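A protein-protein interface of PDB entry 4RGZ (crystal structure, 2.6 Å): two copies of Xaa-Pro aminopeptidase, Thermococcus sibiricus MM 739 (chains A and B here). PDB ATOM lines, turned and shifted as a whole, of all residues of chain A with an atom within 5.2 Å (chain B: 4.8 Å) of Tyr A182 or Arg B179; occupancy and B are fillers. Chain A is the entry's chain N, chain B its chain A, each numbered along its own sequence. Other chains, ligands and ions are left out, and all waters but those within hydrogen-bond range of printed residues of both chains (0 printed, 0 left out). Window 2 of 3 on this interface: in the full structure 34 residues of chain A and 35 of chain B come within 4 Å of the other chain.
OD1 of Asn B178 sits at hydrogen-bond distance from ND2 of Asn A186.
The side-chain hydroxyl (OH) of Tyr A182 sits at hydrogen-bond distance from the guanidinium group (NE) of Arg B179.
OE2 of Glu B181 is in salt-bridge range of NZ of Lys A185 (2.9 Å).
The side-chain amide oxygen (OD1) of Asn A186 sits at hydrogen-bond distance from the side-chain hydroxyl (OH) of Tyr A182 (3.2 Å).
C of Asn A178 touches CE1 of Tyr B182, at 3.999 Å.
Tyr B182 touches Arg A179 (CE1 to N, 3.96 Å).
Tyr A182 touches Asn B178 (O to OD1, 3.7 Å).
Tyr B182 touches Tyr A182 (CB to CD1, 3.9 Å).
CB of Lys A185 touches OD1 of Asn B178, at 2.8 Å.
Asn A186 touches Glu B175.
Tyr A182 touches just these residues of chain B: Asn B178, Arg B179 and Tyr B182.
Of chain A, only Tyr A182 comes within 4 Å of Arg B179.
Of the printed residues of chain B, Arg A179 touches Tyr B182.
Of the printed residues of chain A, Glu B175 touches Asn A186 (3.4 Å).
Printed residues of chain B within 4 Å of Asn A186: Glu B175 (3.4 Å) and Asn B178 (3.4 Å).
Of the printed residues of chain B, Lys A185 touches Asn B178 (2.8 Å) and Glu B181 (2.9 Å).
Of the printed residues of chain A, Glu B181 touches Lys A185 (2.9 Å).
The nearest printed residue of chain B that does not touch Tyr A182 is Glu B175 (4.9 Å).
Hydrophobic or aromatic side chains of chain B that line the printed part of chain A: Tyr B182.
Printed residues of chain A that touch a printed residue of chain B: Asn A178, Arg A179, Tyr A182, Lys A185 and Asn A186.
Along chain A the printed residues that touch a printed residue of chain B span positions 178 to 186.
Among the printed residues, 9 pairs touch across the chains.
Asn A178 touches Tyr B182, and with the chains exchanged Tyr A182 touches Asn B178.
Arg A179 touches Tyr B182, and with the chains exchanged Tyr A182 touches Arg B179.
Tyr A182 touches its own counterpart, Tyr B182.
Positions printed for both chains: 178, 179, 180, 181, 182 and 183.
Of the 9 pairs that touch across the chains among the printed residues, 5 have their exchanged pair printed and touching as well.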
ATOM      1  N   ASN A 178      20.918 -30.984  -9.682  1.00  0.00           N
ATOM      2  CA  ASN A 178      21.776 -30.131 -10.498  1.00  0.00           C
ATOM      3  C   ASN A 178      23.207 -30.166 -10.019  1.00  0.00           C
ATOM      4  O   ASN A 178      24.134 -30.194 -10.850  1.00  0.00           O
ATOM      5  CB  ASN A 178      21.289 -28.686 -10.589  1.00  0.00           C
ATOM      6  CG  ASN A 178      19.940 -28.570 -11.250  1.00  0.00           C
ATOM      7  OD1 ASN A 178      19.511 -29.474 -11.966  1.00  0.00           O
ATOM      8  ND2 ASN A 178      19.248 -27.461 -10.997  1.00  0.00           N
ATOM      9  N   ARG A 179      23.382 -30.175  -8.691  1.00  0.00           N
ATOM     10  CA  ARG A 179      24.723 -30.233  -8.117  1.00  0.00           C
ATOM     11  C   ARG A 179      25.452 -31.560  -8.449  1.00  0.00           C
ATOM     12  O   ARG A 179      26.639 -31.565  -8.788  1.00  0.00           O
ATOM     13  CB  ARG A 179      24.724 -29.832  -6.638  1.00  0.00           C
ATOM     14  CG  ARG A 179      25.048 -30.886  -5.616  1.00  0.00           C
ATOM     15  CD  ARG A 179      25.833 -30.219  -4.491  1.00  0.00           C
ATOM     16  NE  ARG A 179      25.019 -29.638  -3.412  1.00  0.00           N
ATOM     17  CZ  ARG A 179      24.995 -30.103  -2.158  1.00  0.00           C
ATOM     18  NH1 ARG A 179      25.731 -31.161  -1.806  1.00  0.00           N
ATOM     19  NH2 ARG A 179      24.231 -29.518  -1.245  1.00  0.00           N
ATOM     20  N   ILE A 180      24.709 -32.652  -8.446  1.00  0.00           N
ATOM     21  CA  ILE A 180      25.241 -33.916  -8.897  1.00  0.00           C
ATOM     22  C   ILE A 180      25.679 -33.875 -10.368  1.00  0.00           C
ATOM     23  O   ILE A 180      26.744 -34.388 -10.717  1.00  0.00           O
ATOM     24  CB  ILE A 180      24.249 -35.067  -8.710  1.00  0.00           C
ATOM     25  CG1 ILE A 180      23.970 -35.291  -7.211  1.00  0.00           C
ATOM     26  CG2 ILE A 180      24.776 -36.317  -9.432  1.00  0.00           C
ATOM     27  CD1 ILE A 180      23.057 -36.475  -6.933  1.00  0.00           C
ATOM     28  N   GLU A 181      24.872 -33.268 -11.224  1.00  0.00           N
ATOM     29  CA  GLU A 181      25.302 -33.065 -12.609  1.00  0.00           C
ATOM     30  C   GLU A 181      26.588 -32.231 -12.699  1.00  0.00           C
ATOM     31  O   GLU A 181      27.449 -32.508 -13.533  1.00  0.00           O
ATOM     32  CB  GLU A 181      24.210 -32.427 -13.453  1.00  0.00           C
ATOM     33  CG  GLU A 181      24.699 -31.952 -14.801  1.00  0.00           C
ATOM     34  CD  GLU A 181      23.551 -31.591 -15.708  1.00  0.00           C
ATOM     35  OE1 GLU A 181      23.214 -32.440 -16.548  1.00  0.00           O
ATOM     36  OE2 GLU A 181      22.967 -30.481 -15.558  1.00  0.00           O
ATOM     37  N   TYR A 182      26.728 -31.226 -11.847  1.00  0.00           N
ATOM     38  CA  TYR A 182      27.932 -30.385 -11.897  1.00  0.00           C
ATOM     39  C   TYR A 182      29.150 -31.154 -11.373  1.00  0.00           C
ATOM     40  O   TYR A 182      30.255 -30.980 -11.881  1.00  0.00           O
ATOM     41  CB  TYR A 182      27.725 -29.058 -11.166  1.00  0.00           C
ATOM     42  CG  TYR A 182      28.916 -28.126 -11.110  1.00  0.00           C
ATOM     43  CD1 TYR A 182      29.122 -27.167 -12.100  1.00  0.00           C
ATOM     44  CD2 TYR A 182      29.810 -28.161 -10.037  1.00  0.00           C
ATOM     45  CE1 TYR A 182      30.199 -26.282 -12.047  1.00  0.00           C
ATOM     46  CE2 TYR A 182      30.884 -27.298  -9.977  1.00  0.00           C
ATOM     47  CZ  TYR A 182      31.074 -26.360 -10.987  1.00  0.00           C
ATOM     48  OH  TYR A 182      32.135 -25.486 -10.923  1.00  0.00           O
ATOM     49  N   MET A 183      28.923 -32.032 -10.394  1.00  0.00           N
ATOM     50  CA  MET A 183      29.989 -32.828  -9.850  1.00  0.00           C
ATOM     51  C   MET A 183      30.564 -33.752 -10.897  1.00  0.00           C
ATOM     52  O   MET A 183      31.773 -33.744 -11.133  1.00  0.00           O
ATOM     53  CB  MET A 183      29.532 -33.570  -8.608  1.00  0.00           C
ATOM     54  CG  MET A 183      29.753 -32.729  -7.351  1.00  0.00           C
ATOM     55  SD  MET A 183      28.895 -33.397  -5.911  1.00  0.00           S
ATOM     56  CE  MET A 183      29.210 -32.069  -4.746  1.00  0.00           C
ATOM     57  N   ILE A 184      29.688 -34.506 -11.549  1.00  0.00           N
ATOM     58  CA  ILE A 184      30.065 -35.410 -12.614  1.00  0.00           C
ATOM     59  C   ILE A 184      30.901 -34.723 -13.661  1.00  0.00           C
ATOM     60  O   ILE A 184      32.006 -35.162 -13.964  1.00  0.00           O
ATOM     61  CB  ILE A 184      28.810 -36.009 -13.276  1.00  0.00           C
ATOM     62  CG1 ILE A 184      28.024 -36.848 -12.240  1.00  0.00           C
ATOM     63  CG2 ILE A 184      29.164 -36.804 -14.539  1.00  0.00           C
ATOM     64  CD1 ILE A 184      26.696 -37.387 -12.750  1.00  0.00           C
ATOM     65  N   LYS A 185      30.370 -33.641 -14.215  1.00  0.00           N
ATOM     66  CA  LYS A 185      31.024 -32.933 -15.297  1.00  0.00           C
ATOM     67  C   LYS A 185      32.300 -32.191 -14.901  1.00  0.00           C
ATOM     68  O   LYS A 185      33.142 -31.938 -15.750  1.00  0.00           O
ATOM     69  CB  LYS A 185      30.047 -31.959 -15.948  1.00  0.00           C
ATOM     70  CG  LYS A 185      29.020 -32.596 -16.874  1.00  0.00           C
ATOM     71  CD  LYS A 185      28.132 -31.527 -17.520  1.00  0.00           C
ATOM     72  CE  LYS A 185      27.010 -32.203 -18.295  1.00  0.00           C
ATOM     73  NZ  LYS A 185      26.296 -31.363 -19.296  1.00  0.00           N
ATOM     74  N   ASN A 186      32.453 -31.799 -13.644  1.00  0.00           N
ATOM     75  CA  ASN A 186      33.720 -31.193 -13.281  1.00  0.00           C
ATOM     76  C   ASN A 186      34.870 -32.198 -13.082  1.00  0.00           C
ATOM     77  O   ASN A 186      35.930 -31.837 -12.614  1.00  0.00           O
ATOM     78  CB  ASN A 186      33.594 -30.133 -12.174  1.00  0.00           C
ATOM     79  CG  ASN A 186      33.605 -28.702 -12.746  1.00  0.00           C
ATOM     80  OD1 ASN A 186      34.032 -27.749 -12.092  1.00  0.00           O
ATOM     81  ND2 ASN A 186      33.163 -28.558 -13.990  1.00  0.00           N
ATOM     82  N   LYS B 171      40.861 -21.717 -15.535  1.00  0.00           N
ATOM     83  CA  LYS B 171      39.797 -22.685 -15.729  1.00  0.00           C
ATOM     84  C   LYS B 171      39.732 -23.139 -17.160  1.00  0.00           C
ATOM     85  O   LYS B 171      40.030 -22.375 -18.052  1.00  0.00           O
ATOM     86  CB  LYS B 171      38.464 -22.126 -15.248  1.00  0.00           C
ATOM     87  CG  LYS B 171      38.423 -22.027 -13.727  1.00  0.00           C
ATOM     88  CD  LYS B 171      37.294 -21.126 -13.251  1.00  0.00           C
ATOM     89  CE  LYS B 171      37.346 -20.928 -11.748  1.00  0.00           C
ATOM     90  NZ  LYS B 171      37.247 -19.485 -11.387  1.00  0.00           N
ATOM     91  N   GLU B 175      35.030 -26.620 -17.595  1.00  0.00           N
ATOM     92  CA  GLU B 175      34.645 -25.985 -16.344  1.00  0.00           C
ATOM     93  C   GLU B 175      33.759 -24.756 -16.570  1.00  0.00           C
ATOM     94  O   GLU B 175      32.705 -24.640 -15.979  1.00  0.00           O
ATOM     95  CB  GLU B 175      35.877 -25.579 -15.551  1.00  0.00           C
ATOM     96  CG  GLU B 175      36.188 -26.501 -14.397  1.00  0.00           C
ATOM     97  CD  GLU B 175      37.682 -26.749 -14.213  1.00  0.00           C
ATOM     98  OE1 GLU B 175      38.025 -27.696 -13.453  1.00  0.00           O
ATOM     99  OE2 GLU B 175      38.515 -26.021 -14.829  1.00  0.00           O
ATOM    100  N   LEU B 176      34.188 -23.836 -17.417  1.00  0.00           N
ATOM    101  CA  LEU B 176      33.422 -22.662 -17.643  1.00  0.00           C
ATOM    102  C   LEU B 176      32.017 -22.978 -18.202  1.00  0.00           C
ATOM    103  O   LEU B 176      31.001 -22.486 -17.683  1.00  0.00           O
ATOM    104  CB  LEU B 176      34.199 -21.777 -18.562  1.00  0.00           C
ATOM    105  CG  LEU B 176      35.045 -20.679 -17.925  1.00  0.00           C
ATOM    106  CD1 LEU B 176      35.433 -20.828 -16.459  1.00  0.00           C
ATOM    107  CD2 LEU B 176      36.261 -20.461 -18.791  1.00  0.00           C
ATOM    108  N   ALA B 177      31.965 -23.827 -19.230  1.00  0.00           N
ATOM    109  CA  ALA B 177      30.710 -24.390 -19.747  1.00  0.00           C
ATOM    110  C   ALA B 177      29.821 -24.980 -18.632  1.00  0.00           C
ATOM    111  O   ALA B 177      28.610 -24.875 -18.662  1.00  0.00           O
ATOM    112  CB  ALA B 177      30.994 -25.438 -20.815  1.00  0.00           C
ATOM    113  N   ASN B 178      30.436 -25.616 -17.661  1.00  0.00           N
ATOM    114  CA  ASN B 178      29.716 -26.110 -16.519  1.00  0.00           C
ATOM    115  C   ASN B 178      29.162 -25.055 -15.597  1.00  0.00           C
ATOM    116  O   ASN B 178      28.019 -25.216 -15.173  1.00  0.00           O
ATOM    117  CB  ASN B 178      30.591 -27.035 -15.713  1.00  0.00           C
ATOM    118  CG  ASN B 178      30.312 -28.468 -16.017  1.00  0.00           C
ATOM    119  OD1 ASN B 178      30.032 -29.269 -15.110  1.00  0.00           O
ATOM    120  ND2 ASN B 178      30.347 -28.807 -17.315  1.00  0.00           N
ATOM    121  N   ARG B 179      29.953 -24.015 -15.256  1.00  0.00           N
ATOM    122  CA  ARG B 179      29.427 -22.900 -14.418  1.00  0.00           C
ATOM    123  C   ARG B 179      28.188 -22.353 -15.126  1.00  0.00           C
ATOM    124  O   ARG B 179      27.164 -22.158 -14.493  1.00  0.00           O
ATOM    125  CB  ARG B 179      30.391 -21.710 -14.127  1.00  0.00           C
ATOM    126  CG  ARG B 179      31.856 -21.955 -13.779  1.00  0.00           C
ATOM    127  CD  ARG B 179      32.130 -23.013 -12.722  1.00  0.00           C
ATOM    128  NE  ARG B 179      32.450 -22.508 -11.383  1.00  0.00           N
ATOM    129  CZ  ARG B 179      33.677 -22.478 -10.860  1.00  0.00           C
ATOM    130  NH1 ARG B 179      34.723 -22.895 -11.569  1.00  0.00           N
ATOM    131  NH2 ARG B 179      33.866 -22.033  -9.625  1.00  0.00           N
ATOM    132  N   ILE B 180      28.279 -22.154 -16.438  1.00  0.00           N
ATOM    133  CA  ILE B 180      27.192 -21.531 -17.165  1.00  0.00           C
ATOM    134  C   ILE B 180      25.913 -22.365 -17.021  1.00  0.00           C
ATOM    135  O   ILE B 180      24.898 -21.875 -16.549  1.00  0.00           O
ATOM    136  CB  ILE B 180      27.541 -21.236 -18.634  1.00  0.00           C
ATOM    137  CG1 ILE B 180      28.656 -20.197 -18.710  1.00  0.00           C
ATOM    138  CG2 ILE B 180      26.328 -20.722 -19.381  1.00  0.00           C
ATOM    139  CD1 ILE B 180      29.066 -19.826 -20.135  1.00  0.00           C
ATOM    140  N   GLU B 181      25.976 -23.630 -17.387  1.00  0.00           N
ATOM    141  CA  GLU B 181      24.831 -24.502 -17.270  1.00  0.00           C
ATOM    142  C   GLU B 181      24.255 -24.515 -15.856  1.00  0.00           C
ATOM    143  O   GLU B 181      23.032 -24.396 -15.681  1.00  0.00           O
ATOM    144  CB  GLU B 181      25.222 -25.890 -17.715  1.00  0.00           C
ATOM    145  CG  GLU B 181      24.152 -26.924 -17.548  1.00  0.00           C
ATOM    146  CD  GLU B 181      24.383 -28.095 -18.456  1.00  0.00           C
ATOM    147  OE1 GLU B 181      23.421 -28.444 -19.151  1.00  0.00           O
ATOM    148  OE2 GLU B 181      25.512 -28.660 -18.480  1.00  0.00           O
ATOM    149  N   TYR B 182      25.146 -24.629 -14.868  1.00  0.00           N
ATOM    150  CA  TYR B 182      24.773 -24.672 -13.459  1.00  0.00           C
ATOM    151  C   TYR B 182      24.060 -23.408 -13.055  1.00  0.00           C
ATOM    152  O   TYR B 182      23.006 -23.473 -12.425  1.00  0.00           O
ATOM    153  CB  TYR B 182      25.987 -24.850 -12.554  1.00  0.00           C
ATOM    154  CG  TYR B 182      25.607 -25.092 -11.103  1.00  0.00           C
ATOM    155  CD1 TYR B 182      24.966 -26.257 -10.713  1.00  0.00           C
ATOM    156  CD2 TYR B 182      25.864 -24.134 -10.127  1.00  0.00           C
ATOM    157  CE1 TYR B 182      24.610 -26.474  -9.391  1.00  0.00           C
ATOM    158  CE2 TYR B 182      25.503 -24.336  -8.802  1.00  0.00           C
ATOM    159  CZ  TYR B 182      24.881 -25.508  -8.449  1.00  0.00           C
ATOM    160  OH  TYR B 182      24.534 -25.704  -7.146  1.00  0.00           O
ATOM    161  N   MET B 183      24.651 -22.268 -13.399  1.00  0.00           N
ATOM    162  CA  MET B 183      24.007 -20.974 -13.196  1.00  0.00           C
ATOM    163  C   MET B 183      22.586 -20.891 -13.762  1.00  0.00           C
ATOM    164  O   MET B 183      21.654 -20.602 -13.015  1.00  0.00           O
ATOM    165  CB  MET B 183      24.857 -19.844 -13.739  1.00  0.00           C
ATOM    166  CG  MET B 183      25.985 -19.461 -12.805  1.00  0.00           C
ATOM    167  SD  MET B 183      26.824 -18.054 -13.535  1.00  0.00           S
ATOM    168  CE  MET B 183      27.938 -18.795 -14.710  1.00  0.00           C
